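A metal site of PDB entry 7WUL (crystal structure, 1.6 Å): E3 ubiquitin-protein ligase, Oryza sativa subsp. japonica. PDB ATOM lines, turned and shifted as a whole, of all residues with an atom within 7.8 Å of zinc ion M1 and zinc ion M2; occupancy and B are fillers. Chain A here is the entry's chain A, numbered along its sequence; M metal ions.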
ATOM      1  N   ALA A   1       5.662   7.109   8.741  1.00  0.00           N
ATOM      2  CA  ALA A   1       6.926   6.426   9.008  1.00  0.00           C
ATOM      3  C   ALA A   1       7.726   7.112  10.129  1.00  0.00           C
ATOM      4  O   ALA A   1       8.210   6.440  11.034  1.00  0.00           O
ATOM      5  CB  ALA A   1       7.778   6.339   7.733  1.00  0.00           C
ATOM      6  N   VAL A   2       7.874   8.438  10.043  1.00  0.00           N
ATOM      7  CA  VAL A   2       8.644   9.230  10.989  1.00  0.00           C
ATOM      8  C   VAL A   2       7.727  10.308  11.532  1.00  0.00           C
ATOM      9  O   VAL A   2       7.095  11.035  10.750  1.00  0.00           O
ATOM     10  CB  VAL A   2       9.893   9.851  10.337  1.00  0.00           C
ATOM     11  CG1 VAL A   2      10.505  10.916  11.248  1.00  0.00           C
ATOM     12  CG2 VAL A   2      10.909   8.780  10.010  1.00  0.00           C
ATOM     13  N   CYS A   3       7.687  10.440  12.854  1.00  0.00           N
ATOM     14  CA  CYS A   3       6.775  11.386  13.489  1.00  0.00           C
ATOM     15  C   CYS A   3       6.984  12.790  12.922  1.00  0.00           C
ATOM     16  O   CYS A   3       8.092  13.327  12.955  1.00  0.00           O
ATOM     17  CB  CYS A   3       7.021  11.382  14.997  1.00  0.00           C
ATOM     18  SG  CYS A   3       5.921  12.485  15.868  1.00  0.00           S
ATOM     19  N   GLY A   4       5.909  13.393  12.448  1.00  0.00           N
ATOM     20  CA  GLY A   4       6.053  14.738  11.917  1.00  0.00           C
ATOM     21  C   GLY A   4       5.828  15.843  12.935  1.00  0.00           C
ATOM     22  O   GLY A   4       5.582  16.989  12.549  1.00  0.00           O
ATOM     23  N   SER A   5       5.918  15.542  14.228  1.00  0.00           N
ATOM     24  CA  SER A   5       5.532  16.533  15.227  1.00  0.00           C
ATOM     25  C   SER A   5       6.607  17.605  15.370  1.00  0.00           C
ATOM     26  O   SER A   5       7.800  17.319  15.424  1.00  0.00           O
ATOM     27  CB  SER A   5       5.252  15.874  16.575  1.00  0.00           C
ATOM     28  OG  SER A   5       4.576  16.788  17.429  1.00  0.00           O
ATOM     29  N   VAL A   6       6.169  18.852  15.427  1.00  0.00           N
ATOM     30  CA  VAL A   6       7.062  19.968  15.641  1.00  0.00           C
ATOM     31  C   VAL A   6       6.649  20.648  16.936  1.00  0.00           C
ATOM     32  O   VAL A   6       5.488  20.593  17.348  1.00  0.00           O
ATOM     33  CB  VAL A   6       7.036  20.981  14.482  1.00  0.00           C
ATOM     34  CG1 VAL A   6       7.453  20.291  13.196  1.00  0.00           C
ATOM     35  CG2 VAL A   6       5.649  21.574  14.346  1.00  0.00           C
ATOM     36  N   TRP A   7       7.628  21.257  17.602  1.00  0.00           N
ATOM     37  CA  TRP A   7       7.339  22.003  18.815  1.00  0.00           C
ATOM     38  C   TRP A   7       8.230  23.233  18.884  1.00  0.00           C
ATOM     39  O   TRP A   7       9.241  23.354  18.174  1.00  0.00           O
ATOM     40  CB  TRP A   7       7.502  21.137  20.079  1.00  0.00           C
ATOM     41  CG  TRP A   7       8.911  20.653  20.333  1.00  0.00           C
ATOM     42  CD1 TRP A   7       9.872  21.272  21.089  1.00  0.00           C
ATOM     43  CD2 TRP A   7       9.494  19.423  19.879  1.00  0.00           C
ATOM     44  NE1 TRP A   7      11.013  20.513  21.130  1.00  0.00           N
ATOM     45  CE2 TRP A   7      10.815  19.385  20.372  1.00  0.00           C
ATOM     46  CE3 TRP A   7       9.032  18.366  19.080  1.00  0.00           C
ATOM     47  CZ2 TRP A   7      11.675  18.320  20.118  1.00  0.00           C
ATOM     48  CZ3 TRP A   7       9.890  17.322  18.829  1.00  0.00           C
ATOM     49  CH2 TRP A   7      11.199  17.300  19.332  1.00  0.00           C
ATOM     50  N   ALA A  26      15.977  14.413  19.627  1.00  0.00           N
ATOM     51  CA  ALA A  26      14.912  14.556  20.615  1.00  0.00           C
ATOM     52  C   ALA A  26      13.638  13.965  20.046  1.00  0.00           C
ATOM     53  O   ALA A  26      13.430  13.944  18.827  1.00  0.00           O
ATOM     54  CB  ALA A  26      14.661  16.024  20.997  1.00  0.00           C
ATOM     55  N   ILE A  27      12.771  13.506  20.941  1.00  0.00           N
ATOM     56  CA  ILE A  27      11.452  13.037  20.518  1.00  0.00           C
ATOM     57  C   ILE A  27      10.372  13.744  21.322  1.00  0.00           C
ATOM     58  O   ILE A  27      10.613  14.262  22.418  1.00  0.00           O
ATOM     59  CB  ILE A  27      11.295  11.496  20.623  1.00  0.00           C
ATOM     60  CG1 ILE A  27      11.372  11.006  22.082  1.00  0.00           C
ATOM     61  CG2 ILE A  27      12.313  10.796  19.690  1.00  0.00           C
ATOM     62  CD1 ILE A  27      11.093   9.496  22.223  1.00  0.00           C
ATOM     63  N   CYS A  28       9.181  13.812  20.740  1.00  0.00           N
ATOM     64  CA  CYS A  28       8.072  14.537  21.351  1.00  0.00           C
ATOM     65  C   CYS A  28       7.553  13.779  22.577  1.00  0.00           C
ATOM     66  O   CYS A  28       7.808  12.596  22.761  1.00  0.00           O
ATOM     67  CB  CYS A  28       6.951  14.784  20.328  1.00  0.00           C
ATOM     68  SG  CYS A  28       6.011  13.323  19.808  1.00  0.00           S
ATOM     69  N   VAL A  29       6.846  14.503  23.444  1.00  0.00           N
ATOM     70  CA  VAL A  29       6.338  13.869  24.669  1.00  0.00           C
ATOM     71  C   VAL A  29       5.482  12.650  24.354  1.00  0.00           C
ATOM     72  O   VAL A  29       5.708  11.589  24.953  1.00  0.00           O
ATOM     73  CB  VAL A  29       5.605  14.907  25.537  1.00  0.00           C
ATOM     74  CG1 VAL A  29       4.843  14.180  26.652  1.00  0.00           C
ATOM     75  CG2 VAL A  29       6.581  15.903  26.114  1.00  0.00           C
ATOM     76  N   PRO A  30       4.509  12.703  23.431  1.00  0.00           N
ATOM     77  CA  PRO A  30       3.717  11.492  23.206  1.00  0.00           C
ATOM     78  C   PRO A  30       4.520  10.319  22.658  1.00  0.00           C
ATOM     79  O   PRO A  30       4.241   9.165  23.026  1.00  0.00           O
ATOM     80  CB  PRO A  30       2.624  11.949  22.224  1.00  0.00           C
ATOM     81  CG  PRO A  30       2.608  13.403  22.302  1.00  0.00           C
ATOM     82  CD  PRO A  30       3.905  13.897  22.834  1.00  0.00           C
ATOM     83  N   CYS A  31       5.527  10.556  21.816  1.00  0.00           N
ATOM     84  CA  CYS A  31       6.345   9.444  21.337  1.00  0.00           C
ATOM     85  C   CYS A  31       7.168   8.859  22.475  1.00  0.00           C
ATOM     86  O   CYS A  31       7.364   7.639  22.524  1.00  0.00           O
ATOM     87  CB  CYS A  31       7.259   9.881  20.211  1.00  0.00           C
ATOM     88  SG  CYS A  31       6.360  10.034  18.645  1.00  0.00           S
ATOM     89  N   PHE A  32       7.649   9.690  23.399  1.00  0.00           N
ATOM     90  CA  PHE A  32       8.347   9.112  24.547  1.00  0.00           C
ATOM     91  C   PHE A  32       7.406   8.243  25.387  1.00  0.00           C
ATOM     92  O   PHE A  32       7.751   7.109  25.770  1.00  0.00           O
ATOM     93  CB  PHE A  32       8.975  10.218  25.422  1.00  0.00           C
ATOM     94  CG  PHE A  32       9.714   9.664  26.591  1.00  0.00           C
ATOM     95  CD1 PHE A  32       9.085   9.423  27.810  1.00  0.00           C
ATOM     96  CD2 PHE A  32      11.043   9.292  26.441  1.00  0.00           C
ATOM     97  CE1 PHE A  32       9.788   8.851  28.878  1.00  0.00           C
ATOM     98  CE2 PHE A  32      11.730   8.734  27.498  1.00  0.00           C
ATOM     99  CZ  PHE A  32      11.100   8.512  28.706  1.00  0.00           C
ATOM    100  N   ASN A  34       4.730   6.655  24.619  1.00  0.00           N
ATOM    101  CA  ASN A  34       4.297   5.443  23.954  1.00  0.00           C
ATOM    102  C   ASN A  34       5.443   4.525  23.571  1.00  0.00           C
ATOM    103  O   ASN A  34       5.231   3.519  22.882  1.00  0.00           O
ATOM    104  CB  ASN A  34       3.452   5.797  22.729  1.00  0.00           C
ATOM    105  CG  ASN A  34       2.070   6.278  23.120  1.00  0.00           C
ATOM    106  OD1 ASN A  34       1.526   5.852  24.143  1.00  0.00           O
ATOM    107  ND2 ASN A  34       1.516   7.180  22.325  1.00  0.00           N
ATOM    108  N   GLY A  35       6.656   4.840  24.030  1.00  0.00           N
ATOM    109  CA  GLY A  35       7.811   3.997  23.850  1.00  0.00           C
ATOM    110  C   GLY A  35       8.327   3.428  25.170  1.00  0.00           C
ATOM    111  O   GLY A  35       7.780   3.646  26.249  1.00  0.00           O
ATOM    112  N   CYS A  51      11.937  19.082  15.765  1.00  0.00           N
ATOM    113  CA  CYS A  51      11.111  18.151  15.022  1.00  0.00           C
ATOM    114  C   CYS A  51      11.392  16.750  15.517  1.00  0.00           C
ATOM    115  O   CYS A  51      12.559  16.377  15.702  1.00  0.00           O
ATOM    116  CB  CYS A  51      11.410  18.208  13.517  1.00  0.00           C
ATOM    117  SG  CYS A  51      11.113  19.800  12.752  1.00  0.00           S
ATOM    118  N   CYS A  52      10.341  15.962  15.718  1.00  0.00           N
ATOM    119  CA  CYS A  52      10.491  14.681  16.390  1.00  0.00           C
ATOM    120  C   CYS A  52      11.328  13.711  15.545  1.00  0.00           C
ATOM    121  O   CYS A  52      11.146  13.598  14.325  1.00  0.00           O
ATOM    122  CB  CYS A  52       9.112  14.072  16.646  1.00  0.00           C
ATOM    123  SG  CYS A  52       9.208  12.591  17.656  1.00  0.00           S
ATOM    124  N   ASP A  53      12.229  12.991  16.202  1.00  0.00           N
ATOM    125  CA  ASP A  53      13.059  12.001  15.541  1.00  0.00           C
ATOM    126  C   ASP A  53      12.510  10.581  15.622  1.00  0.00           C
ATOM    127  O   ASP A  53      13.159   9.652  15.123  1.00  0.00           O
ATOM    128  CB  ASP A  53      14.471  12.017  16.132  1.00  0.00           C
ATOM    129  CG  ASP A  53      15.226  13.294  15.813  1.00  0.00           C
ATOM    130  OD1 ASP A  53      15.032  13.848  14.708  1.00  0.00           O
ATOM    131  OD2 ASP A  53      15.994  13.747  16.688  1.00  0.00           O
ATOM    132  N   CYS A  54      11.340  10.393  16.225  1.00  0.00           N
ATOM    133  CA  CYS A  54      10.833   9.043  16.418  1.00  0.00           C
ATOM    134  C   CYS A  54      10.497   8.385  15.082  1.00  0.00           C
ATOM    135  O   CYS A  54       9.721   8.930  14.288  1.00  0.00           O
ATOM    136  CB  CYS A  54       9.604   9.080  17.312  1.00  0.00           C
ATOM    137  SG  CYS A  54       8.939   7.465  17.718  1.00  0.00           S
ATOM    138  N   GLY A  55      11.068   7.217  14.847  1.00  0.00           N
ATOM    139  CA  GLY A  55      10.898   6.503  13.592  1.00  0.00           C
ATOM    140  C   GLY A  55      12.017   6.673  12.606  1.00  0.00           C
ATOM    141  O   GLY A  55      12.060   5.959  11.592  1.00  0.00           O
ATOM    142  N   GLY A  64      14.056   2.411  20.554  1.00  0.00           N
ATOM    143  CA  GLY A  64      13.464   3.559  21.188  1.00  0.00           C
ATOM    144  C   GLY A  64      12.315   4.187  20.429  1.00  0.00           C
ATOM    145  O   GLY A  64      11.853   5.266  20.826  1.00  0.00           O
ATOM    146  N   PHE A  65      11.849   3.577  19.340  1.00  0.00           N
ATOM    147  CA  PHE A  65      10.680   4.071  18.626  1.00  0.00           C
ATOM    148  C   PHE A  65       9.414   3.786  19.428  1.00  0.00           C
ATOM    149  O   PHE A  65       9.275   2.732  20.062  1.00  0.00           O
ATOM    150  CB  PHE A  65      10.538   3.402  17.250  1.00  0.00           C
ATOM    151  CG  PHE A  65      11.643   3.714  16.271  1.00  0.00           C
ATOM    152  CD1 PHE A  65      12.580   4.707  16.520  1.00  0.00           C
ATOM    153  CD2 PHE A  65      11.696   3.026  15.058  1.00  0.00           C
ATOM    154  CE1 PHE A  65      13.584   4.973  15.593  1.00  0.00           C
ATOM    155  CE2 PHE A  65      12.689   3.305  14.127  1.00  0.00           C
ATOM    156  CZ  PHE A  65      13.633   4.279  14.395  1.00  0.00           C
ATOM    157  N   CYS A  66       8.466   4.708  19.371  1.00  0.00           N
ATOM    158  CA  CYS A  66       7.189   4.442  20.017  1.00  0.00           C
ATOM    159  C   CYS A  66       6.391   3.415  19.193  1.00  0.00           C
ATOM    160  O   CYS A  66       6.729   3.080  18.056  1.00  0.00           O
ATOM    161  CB  CYS A  66       6.381   5.724  20.204  1.00  0.00           C
ATOM    162  SG  CYS A  66       5.425   6.273  18.759  1.00  0.00           S
ATOM    163  N   SER A  67       5.320   2.916  19.813  1.00  0.00           N
ATOM    164  CA  SER A  67       4.521   1.869  19.181  1.00  0.00           C
ATOM    165  C   SER A  67       3.883   2.315  17.860  1.00  0.00           C
ATOM    166  O   SER A  67       3.535   1.454  17.047  1.00  0.00           O
ATOM    167  CB  SER A  67       3.441   1.401  20.156  1.00  0.00           C
ATOM    168  OG  SER A  67       2.691   2.498  20.658  1.00  0.00           O
ATOM    169  N   ARG A  68       3.771   3.616  17.621  1.00  0.00           N
ATOM    170  CA  ARG A  68       3.058   4.166  16.470  1.00  0.00           C
ATOM    171  C   ARG A  68       3.968   4.479  15.288  1.00  0.00           C
ATOM    172  O   ARG A  68       3.453   4.695  14.188  1.00  0.00           O
ATOM    173  CB  ARG A  68       2.297   5.431  16.888  1.00  0.00           C
ATOM    174  CG  ARG A  68       1.247   5.117  17.951  1.00  0.00           C
ATOM    175  CD  ARG A  68       0.340   6.276  18.363  1.00  0.00           C
ATOM    176  NE  ARG A  68      -0.348   6.875  17.233  1.00  0.00           N
ATOM    177  CZ  ARG A  68       0.038   7.990  16.635  1.00  0.00           C
ATOM    178  NH1 ARG A  68       1.034   8.711  17.115  1.00  0.00           N
ATOM    179  NH2 ARG A  68      -0.590   8.387  15.535  1.00  0.00           N
ATOM    180  N   HIS A  69       5.286   4.541  15.494  1.00  0.00           N
ATOM    181  CA  HIS A  69       6.250   4.719  14.415  1.00  0.00           C
ATOM    182  C   HIS A  69       7.273   3.585  14.411  1.00  0.00           C
ATOM    183  O   HIS A  69       8.407   3.769  13.965  1.00  0.00           O
ATOM    184  CB  HIS A  69       6.910   6.099  14.473  1.00  0.00           C
ATOM    185  CG  HIS A  69       5.933   7.218  14.657  1.00  0.00           C
ATOM    186  ND1 HIS A  69       5.810   7.931  15.839  1.00  0.00           N
ATOM    187  CD2 HIS A  69       5.016   7.731  13.807  1.00  0.00           C
ATOM    188  CE1 HIS A  69       4.853   8.831  15.698  1.00  0.00           C
ATOM    189  NE2 HIS A  69       4.359   8.734  14.472  1.00  0.00           N
ATOM    190  N   LYS A  70       6.866   2.412  14.881  1.00  0.00           N
ATOM    191  CA  LYS A  70       7.714   1.218  14.846  1.00  0.00           C
ATOM    192  C   LYS A  70       7.164   0.225  13.839  1.00  0.00           C
ATOM    193  O   LYS A  70       7.014   0.553  12.659  1.00  0.00           O
ATOM    194  CB  LYS A  70       7.815   0.593  16.239  1.00  0.00           C
ATOM    195  CG  LYS A  70       6.760  -0.461  16.542  1.00  0.00           C
ATOM    196  CD  LYS A  70       6.918  -0.957  17.986  1.00  0.00           C
ATOM    197  CE  LYS A  70       5.823  -1.954  18.376  1.00  0.00           C
ATOM    198  NZ  LYS A  70       5.767  -2.159  19.856  1.00  0.00           N
HETATM  199 ZN    ZN M   1       6.688   7.880  17.722  1.00  0.00          ZN
HETATM  200 ZN    ZN M   2       6.921  12.243  17.950  1.00  0.00          ZN
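Along chain A the residues within 4 Å of zinc ion M1 span positions 31 to 69.
O of Cys 54 is in hydrogen-bond range of N of Cys 3 (2.9 Å). N of Cys 54 lies close to SG of Cys 52 (3.4 Å). The side-chain sulfur of Cys 66 sits close to the backbone NH of Arg 68 (3.3 Å). N of Ser 5 lies close to SG of Cys 3. N of Cys 52 lies within hydrogen-bond range of O of Ser 5, at 2.9 Å.
Zinc ion M1 is bound by a ring nitrogen (ND1) of His 69 (2.1 Å). The side-chain sulfur (SG) of Cys 54 is bound to zinc ion M1 (2.3 Å). SG of Cys 66 binds zinc ion M1, at 2.3 Å. Zinc ion M1 is bound by the side-chain sulfur (SG) of Cys 31 (2.4 Å).
Zinc ion M2 is bound by the side-chain sulfur of Cys 3 (2.3 Å), the side-chain sulfur of Cys 52 (2.3 Å), the side-chain sulfur of Cys 28 (2.3 Å) and the side-chain sulfur of Cys 31 (2.4 Å). Zinc ion M2 has four donor atoms within binding distance.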
